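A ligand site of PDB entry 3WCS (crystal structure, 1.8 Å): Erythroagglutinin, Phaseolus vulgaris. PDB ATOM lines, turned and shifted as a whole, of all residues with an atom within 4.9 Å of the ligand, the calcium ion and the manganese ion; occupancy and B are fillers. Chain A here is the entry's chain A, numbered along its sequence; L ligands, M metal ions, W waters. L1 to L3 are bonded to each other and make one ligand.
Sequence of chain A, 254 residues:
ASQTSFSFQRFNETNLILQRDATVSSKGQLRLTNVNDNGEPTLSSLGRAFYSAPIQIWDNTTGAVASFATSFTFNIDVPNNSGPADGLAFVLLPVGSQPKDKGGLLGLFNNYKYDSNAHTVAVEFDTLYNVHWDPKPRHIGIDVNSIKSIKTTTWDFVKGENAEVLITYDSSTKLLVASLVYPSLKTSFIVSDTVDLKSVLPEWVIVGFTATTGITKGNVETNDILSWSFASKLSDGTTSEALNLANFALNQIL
N of Ile 215 sits at hydrogen-bond distance from O4 of LG2 L2, 3.2 Å away. The side-chain amide nitrogen (ND2) of Asn 130 sits at hydrogen-bond distance from an oxygen (O5) of LG2 L2 (3.0 Å). ND2 of Asn 219 sits at hydrogen-bond distance from O1 of LG3 L3 (3.0 Å). N of Thr 216 sits at hydrogen-bond distance from O4 of LG2 L2, 3.2 Å away. The backbone NH (N) of Gly 104 is in hydrogen-bond range of an oxygen (O3) of LIG L1 (2.8 Å). The side-chain hydroxyl (OG1) of Thr 216 sits at hydrogen-bond distance from an oxygen (O4) of LG2 L2, 3.5 Å away.
ND2 of Asn 219 sits at hydrogen-bond distance from O of Thr 216 (3.2 Å). N of Gly 214 sits close to O of Asn 219 (3.2 Å). The backbone NH of Gly 104 sits close to the side-chain carboxylate of Asp 86, at 3.5 Å. OD1 of Asp 134 sits close to NE1 of Trp 133 (3.4 Å).
Residues that only touch the ligand: Gly 103, Leu 105, Tyr 129, Val 131, His 132, Trp 133 and Gly 214. Hydrophobic or aromatic side chains within 4 Å of the ligand: Leu 105, Leu 128, Tyr 129, Val 131, His 132, Trp 133 and Ile 215.
Of the 23 residues printed, 4 come within 4 Å of the calcium ion. The nearest printed residue that does not touch the calcium ion is Trp 133 (4.3 Å).
Four residues have an atom within 4 Å of the manganese ion: Glu 124, Asp 126, Asp 134 and His 139. The nearest printed residue that does not touch the manganese ion is Ser 149 (4.3 Å).
The calcium ion is bound by water W1 (2.3 Å). OD2 of Asp 134 binds the calcium ion (2.3 Å). The calcium ion is bound by water W14, at 2.3 Å. The calcium ion is bound by OD1 of Asp 126 (2.3 Å). The calcium ion is bound by OD1 of Asn 130. The calcium ion is bound by the backbone carbonyl oxygen (O) of Leu 128 (2.4 Å). The side-chain carboxylate (OD2) of Asp 126 is bound to the calcium ion.
The manganese ion is bound by water W5, at 2.0 Å. Water W12 binds the manganese ion (2.0 Å). The manganese ion is bound by OD1 of Asp 134 (2.0 Å). NE2 of His 139 binds the manganese ion, 2.0 Å away. The manganese ion is bound by the side-chain carboxylate (OE2) of Glu 124. The manganese ion is bound by OD2 of Asp 126 (2.0 Å). The manganese ion has six donor atoms within binding distance.
Water W14 lies within hydrogen-bond range of O of Gly 104 (3.0 Å) and NE1 of Trp 133 (3.1 Å). Water W5 lies within hydrogen-bond range of OE1 of Glu 124 (2.7 Å), O of Ile 147 (3.1 Å) and NE1 of Trp 133 (3.4 Å). Water W11 lies within hydrogen-bond range of an oxygen (O1) of LG2 L2 (2.7 Å), the backbone carbonyl oxygen of Tyr 129 (2.7 Å) and the backbone NH of Val 131 (3.0 Å). Water W6 lies within hydrogen-bond range of O4 of LIG L1 (2.7 Å) and O of Lys 102 (2.7 Å). Water W4 bridges an oxygen (O5) of LG3 L3 (2.7 Å) and the backbone NH of Tyr 129 (2.9 Å). Water W10 lies within hydrogen-bond range of O4 of LG2 L2 (2.8 Å), OD2 of Asp 86 (2.8 Å) and N of Ile 215 (2.8 Å).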
ATOM      1  N   ASP A  86      17.884   5.768 -30.643  1.00  0.00           N
ATOM      2  CA  ASP A  86      17.706   5.671 -29.168  1.00  0.00           C
ATOM      3  C   ASP A  86      16.841   4.482 -28.791  1.00  0.00           C
ATOM      4  O   ASP A  86      16.831   4.038 -27.621  1.00  0.00           O
ATOM      5  CB  ASP A  86      17.013   6.937 -28.659  1.00  0.00           C
ATOM      6  CG  ASP A  86      17.984   7.984 -28.220  1.00  0.00           C
ATOM      7  OD1 ASP A  86      18.538   7.831 -27.096  1.00  0.00           O
ATOM      8  OD2 ASP A  86      18.166   8.987 -28.955  1.00  0.00           O
ATOM      9  N   LYS A 102      12.036  14.225 -28.296  1.00  0.00           N
ATOM     10  CA  LYS A 102      12.772  13.230 -29.077  1.00  0.00           C
ATOM     11  C   LYS A 102      13.942  12.591 -28.315  1.00  0.00           C
ATOM     12  O   LYS A 102      14.023  12.657 -27.072  1.00  0.00           O
ATOM     13  CB  LYS A 102      13.248  13.867 -30.389  1.00  0.00           C
ATOM     14  CG  LYS A 102      14.265  14.997 -30.201  1.00  0.00           C
ATOM     15  CD  LYS A 102      14.791  15.519 -31.540  1.00  0.00           C
ATOM     16  CE  LYS A 102      13.904  16.624 -32.096  1.00  0.00           C
ATOM     17  NZ  LYS A 102      14.318  16.994 -33.482  1.00  0.00           N
ATOM     18  N   GLY A 103      14.838  11.942 -29.053  1.00  0.00           N
ATOM     19  CA  GLY A 103      16.007  11.302 -28.423  1.00  0.00           C
ATOM     20  C   GLY A 103      15.642  10.253 -27.370  1.00  0.00           C
ATOM     21  O   GLY A 103      14.781   9.408 -27.576  1.00  0.00           O
ATOM     22  N   GLY A 104      16.299  10.343 -26.202  1.00  0.00           N
ATOM     23  CA  GLY A 104      16.102   9.335 -25.170  1.00  0.00           C
ATOM     24  C   GLY A 104      14.703   9.315 -24.546  1.00  0.00           C
ATOM     25  O   GLY A 104      14.356   8.406 -23.832  1.00  0.00           O
ATOM     26  N   LEU A 105      13.914  10.338 -24.802  1.00  0.00           N
ATOM     27  CA  LEU A 105      12.555  10.364 -24.280  1.00  0.00           C
ATOM     28  C   LEU A 105      11.554   9.671 -25.231  1.00  0.00           C
ATOM     29  O   LEU A 105      10.359   9.548 -24.913  1.00  0.00           O
ATOM     30  CB  LEU A 105      12.153  11.808 -23.977  1.00  0.00           C
ATOM     31  CG  LEU A 105      13.027  12.460 -22.877  1.00  0.00           C
ATOM     32  CD1 LEU A 105      12.740  13.953 -22.735  1.00  0.00           C
ATOM     33  CD2 LEU A 105      12.904  11.724 -21.550  1.00  0.00           C
ATOM     34  N   TYR A 112      12.302  13.429 -17.622  1.00  0.00           N
ATOM     35  CA  TYR A 112      12.420  12.082 -17.062  1.00  0.00           C
ATOM     36  C   TYR A 112      11.773  11.887 -15.683  1.00  0.00           C
ATOM     37  O   TYR A 112      12.089  10.933 -14.979  1.00  0.00           O
ATOM     38  CB  TYR A 112      13.869  11.580 -17.088  1.00  0.00           C
ATOM     39  CG  TYR A 112      14.929  12.476 -16.461  1.00  0.00           C
ATOM     40  CD1 TYR A 112      15.322  12.311 -15.127  1.00  0.00           C
ATOM     41  CD2 TYR A 112      15.581  13.447 -17.222  1.00  0.00           C
ATOM     42  CE1 TYR A 112      16.317  13.115 -14.560  1.00  0.00           C
ATOM     43  CE2 TYR A 112      16.585  14.248 -16.675  1.00  0.00           C
ATOM     44  CZ  TYR A 112      16.937  14.081 -15.348  1.00  0.00           C
ATOM     45  OH  TYR A 112      17.936  14.885 -14.843  1.00  0.00           O
ATOM     46  N   GLU A 124       9.469  -0.708 -24.042  1.00  0.00           N
ATOM     47  CA  GLU A 124      10.582  -0.092 -24.757  1.00  0.00           C
ATOM     48  C   GLU A 124      11.723  -1.048 -25.040  1.00  0.00           C
ATOM     49  O   GLU A 124      11.974  -1.984 -24.272  1.00  0.00           O
ATOM     50  CB  GLU A 124      11.126   1.133 -24.014  1.00  0.00           C
ATOM     51  CG  GLU A 124      11.737   0.820 -22.625  1.00  0.00           C
ATOM     52  CD  GLU A 124      12.586   1.973 -22.070  1.00  0.00           C
ATOM     53  OE1 GLU A 124      12.025   3.102 -22.008  1.00  0.00           O
ATOM     54  OE2 GLU A 124      13.796   1.800 -21.702  1.00  0.00           O
ATOM     55  N   ASP A 126      15.358  -0.351 -25.725  1.00  0.00           N
ATOM     56  CA  ASP A 126      16.187   0.872 -25.495  1.00  0.00           C
ATOM     57  C   ASP A 126      17.650   0.528 -25.802  1.00  0.00           C
ATOM     58  O   ASP A 126      18.240  -0.349 -25.165  1.00  0.00           O
ATOM     59  CB  ASP A 126      15.993   1.322 -24.014  1.00  0.00           C
ATOM     60  CG  ASP A 126      16.619   2.697 -23.679  1.00  0.00           C
ATOM     61  OD1 ASP A 126      17.434   3.168 -24.496  1.00  0.00           O
ATOM     62  OD2 ASP A 126      16.278   3.315 -22.589  1.00  0.00           O
ATOM     63  N   LEU A 128      20.230   2.876 -26.048  1.00  0.00           N
ATOM     64  CA  LEU A 128      21.158   3.939 -25.628  1.00  0.00           C
ATOM     65  C   LEU A 128      21.008   4.220 -24.135  1.00  0.00           C
ATOM     66  O   LEU A 128      19.942   4.582 -23.652  1.00  0.00           O
ATOM     67  CB  LEU A 128      20.929   5.224 -26.433  1.00  0.00           C
ATOM     68  CG  LEU A 128      22.099   6.159 -26.024  1.00  0.00           C
ATOM     69  CD1 LEU A 128      23.101   6.521 -27.115  1.00  0.00           C
ATOM     70  CD2 LEU A 128      21.667   7.297 -25.090  1.00  0.00           C
ATOM     71  N   TYR A 129      22.128   4.067 -23.426  1.00  0.00           N
ATOM     72  CA  TYR A 129      22.165   4.348 -21.970  1.00  0.00           C
ATOM     73  C   TYR A 129      22.063   5.840 -21.671  1.00  0.00           C
ATOM     74  O   TYR A 129      22.965   6.618 -22.026  1.00  0.00           O
ATOM     75  CB  TYR A 129      23.465   3.778 -21.434  1.00  0.00           C
ATOM     76  CG  TYR A 129      23.893   4.289 -20.059  1.00  0.00           C
ATOM     77  CD1 TYR A 129      23.080   4.125 -18.966  1.00  0.00           C
ATOM     78  CD2 TYR A 129      25.094   4.962 -19.906  1.00  0.00           C
ATOM     79  CE1 TYR A 129      23.499   4.588 -17.704  1.00  0.00           C
ATOM     80  CE2 TYR A 129      25.521   5.432 -18.667  1.00  0.00           C
ATOM     81  CZ  TYR A 129      24.717   5.247 -17.581  1.00  0.00           C
ATOM     82  OH  TYR A 129      25.154   5.726 -16.344  1.00  0.00           O
ATOM     83  N   ASN A 130      20.973   6.240 -21.008  1.00  0.00           N
ATOM     84  CA  ASN A 130      20.756   7.635 -20.663  1.00  0.00           C
ATOM     85  C   ASN A 130      21.079   7.725 -19.181  1.00  0.00           C
ATOM     86  O   ASN A 130      20.377   7.169 -18.349  1.00  0.00           O
ATOM     87  CB  ASN A 130      19.309   8.058 -20.949  1.00  0.00           C
ATOM     88  CG  ASN A 130      19.042   8.242 -22.439  1.00  0.00           C
ATOM     89  OD1 ASN A 130      18.412   7.384 -23.090  1.00  0.00           O
ATOM     90  ND2 ASN A 130      19.512   9.375 -22.976  1.00  0.00           N
ATOM     91  N   VAL A 131      22.182   8.399 -18.877  1.00  0.00           N
ATOM     92  CA  VAL A 131      22.766   8.384 -17.523  1.00  0.00           C
ATOM     93  C   VAL A 131      21.820   8.722 -16.376  1.00  0.00           C
ATOM     94  O   VAL A 131      21.967   8.203 -15.259  1.00  0.00           O
ATOM     95  CB  VAL A 131      24.032   9.293 -17.495  1.00  0.00           C
ATOM     96  CG1 VAL A 131      23.678  10.748 -17.777  1.00  0.00           C
ATOM     97  CG2 VAL A 131      24.775   9.155 -16.176  1.00  0.00           C
ATOM     98  N   HIS A 132      20.843   9.578 -16.630  1.00  0.00           N
ATOM     99  CA  HIS A 132      19.971  10.060 -15.543  1.00  0.00           C
ATOM    100  C   HIS A 132      18.853   9.129 -15.154  1.00  0.00           C
ATOM    101  O   HIS A 132      18.179   9.333 -14.131  1.00  0.00           O
ATOM    102  CB  HIS A 132      19.434  11.455 -15.850  1.00  0.00           C
ATOM    103  CG  HIS A 132      20.511  12.500 -16.020  1.00  0.00           C
ATOM    104  ND1 HIS A 132      21.427  12.777 -15.057  1.00  0.00           N
ATOM    105  CD2 HIS A 132      20.757  13.395 -17.069  1.00  0.00           C
ATOM    106  CE1 HIS A 132      22.251  13.755 -15.479  1.00  0.00           C
ATOM    107  NE2 HIS A 132      21.844  14.148 -16.715  1.00  0.00           N
ATOM    108  N   TRP A 133      18.613   8.076 -15.951  1.00  0.00           N
ATOM    109  CA  TRP A 133      17.528   7.134 -15.644  1.00  0.00           C
ATOM    110  C   TRP A 133      17.672   5.680 -16.024  1.00  0.00           C
ATOM    111  O   TRP A 133      17.011   4.841 -15.456  1.00  0.00           O
ATOM    112  CB  TRP A 133      16.189   7.675 -16.161  1.00  0.00           C
ATOM    113  CG  TRP A 133      16.114   7.699 -17.673  1.00  0.00           C
ATOM    114  CD1 TRP A 133      15.810   6.637 -18.514  1.00  0.00           C
ATOM    115  CD2 TRP A 133      16.282   8.853 -18.543  1.00  0.00           C
ATOM    116  NE1 TRP A 133      15.826   7.047 -19.841  1.00  0.00           N
ATOM    117  CE2 TRP A 133      16.084   8.367 -19.922  1.00  0.00           C
ATOM    118  CE3 TRP A 133      16.595  10.198 -18.348  1.00  0.00           C
ATOM    119  CZ2 TRP A 133      16.187   9.202 -21.009  1.00  0.00           C
ATOM    120  CZ3 TRP A 133      16.696  11.029 -19.455  1.00  0.00           C
ATOM    121  CH2 TRP A 133      16.504  10.535 -20.762  1.00  0.00           C
ATOM    122  N   ASP A 134      18.500   5.363 -17.022  1.00  0.00           N
ATOM    123  CA  ASP A 134      18.602   3.989 -17.534  1.00  0.00           C
ATOM    124  C   ASP A 134      19.604   3.101 -16.779  1.00  0.00           C
ATOM    125  O   ASP A 134      20.614   3.607 -16.308  1.00  0.00           O
ATOM    126  CB  ASP A 134      19.072   4.014 -19.002  1.00  0.00           C
ATOM    127  CG  ASP A 134      17.924   4.251 -20.006  1.00  0.00           C
ATOM    128  OD1 ASP A 134      16.753   3.785 -19.809  1.00  0.00           O
ATOM    129  OD2 ASP A 134      18.264   4.864 -21.059  1.00  0.00           O
ATOM    130  N   PRO A 135      19.362   1.763 -16.747  1.00  0.00           N
ATOM    131  CA  PRO A 135      20.425   0.805 -16.454  1.00  0.00           C
ATOM    132  C   PRO A 135      21.446   0.876 -17.592  1.00  0.00           C
ATOM    133  O   PRO A 135      21.090   1.236 -18.716  1.00  0.00           O
ATOM    134  CB  PRO A 135      19.709  -0.549 -16.440  1.00  0.00           C
ATOM    135  CG  PRO A 135      18.478  -0.357 -17.267  1.00  0.00           C
ATOM    136  CD  PRO A 135      18.106   1.093 -17.191  1.00  0.00           C
ATOM    137  N   HIS A 139      18.378  -2.742 -22.956  1.00  0.00           N
ATOM    138  CA  HIS A 139      17.334  -3.350 -22.137  1.00  0.00           C
ATOM    139  C   HIS A 139      15.970  -3.294 -22.778  1.00  0.00           C
ATOM    140  O   HIS A 139      15.692  -2.434 -23.633  1.00  0.00           O
ATOM    141  CB  HIS A 139      17.291  -2.665 -20.738  1.00  0.00           C
ATOM    142  CG  HIS A 139      17.159  -1.156 -20.774  1.00  0.00           C
ATOM    143  ND1 HIS A 139      18.216  -0.336 -20.957  1.00  0.00           N
ATOM    144  CD2 HIS A 139      16.020  -0.334 -20.703  1.00  0.00           C
ATOM    145  CE1 HIS A 139      17.789   0.950 -20.952  1.00  0.00           C
ATOM    146  NE2 HIS A 139      16.426   0.966 -20.814  1.00  0.00           N
ATOM    147  N   ILE A 147       9.682   7.687 -18.407  1.00  0.00           N
ATOM    148  CA  ILE A 147      10.797   7.073 -19.149  1.00  0.00           C
ATOM    149  C   ILE A 147      11.655   6.199 -18.221  1.00  0.00           C
ATOM    150  O   ILE A 147      12.427   5.357 -18.683  1.00  0.00           O
ATOM    151  CB  ILE A 147      11.650   8.121 -19.909  1.00  0.00           C
ATOM    152  CG1 ILE A 147      12.481   7.471 -21.027  1.00  0.00           C
ATOM    153  CG2 ILE A 147      12.611   8.834 -18.949  1.00  0.00           C
ATOM    154  CD1 ILE A 147      11.659   6.930 -22.200  1.00  0.00           C
ATOM    155  N   SER A 149      11.824   3.167 -16.410  1.00  0.00           N
ATOM    156  CA  SER A 149      10.998   1.936 -16.497  1.00  0.00           C
ATOM    157  C   SER A 149      10.697   1.395 -15.124  1.00  0.00           C
ATOM    158  O   SER A 149      11.576   1.421 -14.270  1.00  0.00           O
ATOM    159  CB  SER A 149      11.723   0.858 -17.294  1.00  0.00           C
ATOM    160  OG  SER A 149      12.033   1.351 -18.589  1.00  0.00           O
ATOM    161  N   GLY A 214      19.349   9.035 -32.330  1.00  0.00           N
ATOM    162  CA  GLY A 214      20.190   9.842 -31.455  1.00  0.00           C
ATOM    163  C   GLY A 214      20.290  11.278 -31.937  1.00  0.00           C
ATOM    164  O   GLY A 214      20.169  11.552 -33.139  1.00  0.00           O
ATOM    165  N   ILE A 215      20.502  12.198 -31.015  1.00  0.00           N
ATOM    166  CA  ILE A 215      20.641  13.599 -31.403  1.00  0.00           C
ATOM    167  C   ILE A 215      22.098  13.990 -31.675  1.00  0.00           C
ATOM    168  O   ILE A 215      22.364  15.040 -32.252  1.00  0.00           O
ATOM    169  CB  ILE A 215      19.965  14.568 -30.410  1.00  0.00           C
ATOM    170  CG1 ILE A 215      20.653  14.541 -29.023  1.00  0.00           C
ATOM    171  CG2 ILE A 215      18.486  14.247 -30.270  1.00  0.00           C
ATOM    172  CD1 ILE A 215      20.256  15.712 -28.138  1.00  0.00           C
ATOM    173  N   THR A 216      23.029  13.127 -31.263  1.00  0.00           N
ATOM    174  CA  THR A 216      24.463  13.393 -31.360  1.00  0.00           C
ATOM    175  C   THR A 216      25.105  12.469 -32.387  1.00  0.00           C
ATOM    176  O   THR A 216      24.893  11.244 -32.346  1.00  0.00           O
ATOM    177  CB  THR A 216      25.150  13.159 -30.001  1.00  0.00           C
ATOM    178  OG1 THR A 216      24.544  14.015 -29.027  1.00  0.00           O
ATOM    179  CG2 THR A 216      26.636  13.459 -30.078  1.00  0.00           C
ATOM    180  N   ASN A 219      25.471   8.213 -32.920  1.00  0.00           N
ATOM    181  CA  ASN A 219      24.410   7.487 -32.202  1.00  0.00           C
ATOM    182  C   ASN A 219      23.138   7.544 -33.045  1.00  0.00           C
ATOM    183  O   ASN A 219      22.406   8.522 -33.015  1.00  0.00           O
ATOM    184  CB  ASN A 219      24.133   8.140 -30.839  1.00  0.00           C
ATOM    185  CG  ASN A 219      25.392   8.255 -29.992  1.00  0.00           C
ATOM    186  OD1 ASN A 219      25.758   7.312 -29.294  1.00  0.00           O
ATOM    187  ND2 ASN A 219      26.063   9.393 -30.080  1.00  0.00           N
HETATM  188  C1  LIG L   1      20.283  14.724 -24.059  1.00  0.00           C
HETATM  189  C2  LIG L   1      20.122  13.538 -25.005  1.00  0.00           C
HETATM  190  C3  LIG L   1      18.623  13.236 -25.191  1.00  0.00           C
HETATM  191  C4  LIG L   1      17.985  12.936 -23.837  1.00  0.00           C
HETATM  192  C5  LIG L   1      18.192  14.156 -22.941  1.00  0.00           C
HETATM  193  C6  LIG L   1      17.606  13.986 -21.541  1.00  0.00           C
HETATM  194  O1  LIG L   1      19.783  15.902 -24.661  1.00  0.00           O
HETATM  195  O2  LIG L   1      20.701  12.389 -24.425  1.00  0.00           O
HETATM  196  O3  LIG L   1      18.501  12.108 -26.037  1.00  0.00           O
HETATM  197  O4  LIG L   1      16.603  12.607 -23.957  1.00  0.00           O
HETATM  198  O5  LIG L   1      19.593  14.432 -22.834  1.00  0.00           O
HETATM  199  O6  LIG L   1      17.630  15.245 -20.880  1.00  0.00           O
HETATM  200  C1  LG2 L   2      22.060  12.185 -24.858  1.00  0.00           C
HETATM  201  C2  LG2 L   2      22.794  11.483 -23.712  1.00  0.00           C
HETATM  202  C3  LG2 L   2      24.226  11.181 -24.136  1.00  0.00           C
HETATM  203  C4  LG2 L   2      24.286  10.427 -25.464  1.00  0.00           C
HETATM  204  C5  LG2 L   2      23.449  11.159 -26.524  1.00  0.00           C
HETATM  205  C6  LG2 L   2      23.322  10.365 -27.819  1.00  0.00           C
HETATM  206  C7  LG2 L   2      22.043  12.149 -21.476  1.00  0.00           C
HETATM  207  C8  LG2 L   2      22.169  13.175 -20.380  1.00  0.00           C
HETATM  208  N1  LG2 L   2      22.787  12.364 -22.551  1.00  0.00           N
HETATM  209  O1  LG2 L   2      24.878  10.446 -23.120  1.00  0.00           O
HETATM  210  O2  LG2 L   2      25.659  10.414 -25.837  1.00  0.00           O
HETATM  211  O3  LG2 L   2      22.134  11.393 -26.039  1.00  0.00           O
HETATM  212  O4  LG2 L   2      22.567  11.142 -28.741  1.00  0.00           O
HETATM  213  O5  LG2 L   2      21.273  11.187 -21.346  1.00  0.00           O
HETATM  214  C1  LG3 L   3      26.130   9.104 -26.137  1.00  0.00           C
HETATM  215  C2  LG3 L   3      27.599   9.233 -26.530  1.00  0.00           C
HETATM  216  C3  LG3 L   3      28.191   7.840 -26.726  1.00  0.00           C
HETATM  217  C4  LG3 L   3      27.930   6.962 -25.506  1.00  0.00           C
HETATM  218  C5  LG3 L   3      26.435   6.925 -25.166  1.00  0.00           C
HETATM  219  C6  LG3 L   3      26.120   6.202 -23.854  1.00  0.00           C
HETATM  220  O1  LG3 L   3      27.726  10.046 -27.688  1.00  0.00           O
HETATM  221  O2  LG3 L   3      29.585   7.942 -26.957  1.00  0.00           O
HETATM  222  O3  LG3 L   3      28.615   7.519 -24.395  1.00  0.00           O
HETATM  223  O4  LG3 L   3      25.990   8.254 -25.013  1.00  0.00           O
HETATM  224  O5  LG3 L   3      26.435   4.838 -23.887  1.00  0.00           O
HETATM  225 CA    CA M   1      17.689   5.158 -23.281  1.00  0.00          CA
HETATM  226 MN    MN M   2      15.397   2.715 -20.850  1.00  0.00          MN
HETATM  227  O   HOH W   1      17.392   5.691 -25.505  1.00  0.00           O
HETATM  228  O   HOH W   2      24.561  14.588 -22.615  1.00  0.00           O
HETATM  229  O   HOH W   3      19.715  15.915 -19.158  1.00  0.00           O
HETATM  230  O   HOH W   4      24.554   3.036 -24.725  1.00  0.00           O
HETATM  231  O   HOH W   5      14.182   4.252 -20.979  1.00  0.00           O
HETATM  232  O   HOH W   6      15.264  14.459 -25.416  1.00  0.00           O
HETATM  233  O   HOH W   7      15.046  15.681 -19.859  1.00  0.00           O
HETATM  234  O   HOH W   8      27.636   9.614 -22.823  1.00  0.00           O
HETATM  235  O   HOH W   9      19.909  10.929 -19.020  1.00  0.00           O
HETATM  236  O   HOH W  10      19.801  11.206 -28.447  1.00  0.00           O
HETATM  237  O   HOH W  11      24.130   8.900 -21.039  1.00  0.00           O
HETATM  238  O   HOH W  12      14.724   2.402 -18.993  1.00  0.00           O
HETATM  239  O   HOH W  13      19.650   9.699 -25.642  1.00  0.00           O
HETATM  240  O   HOH W  14      15.561   5.939 -22.721  1.00  0.00           O
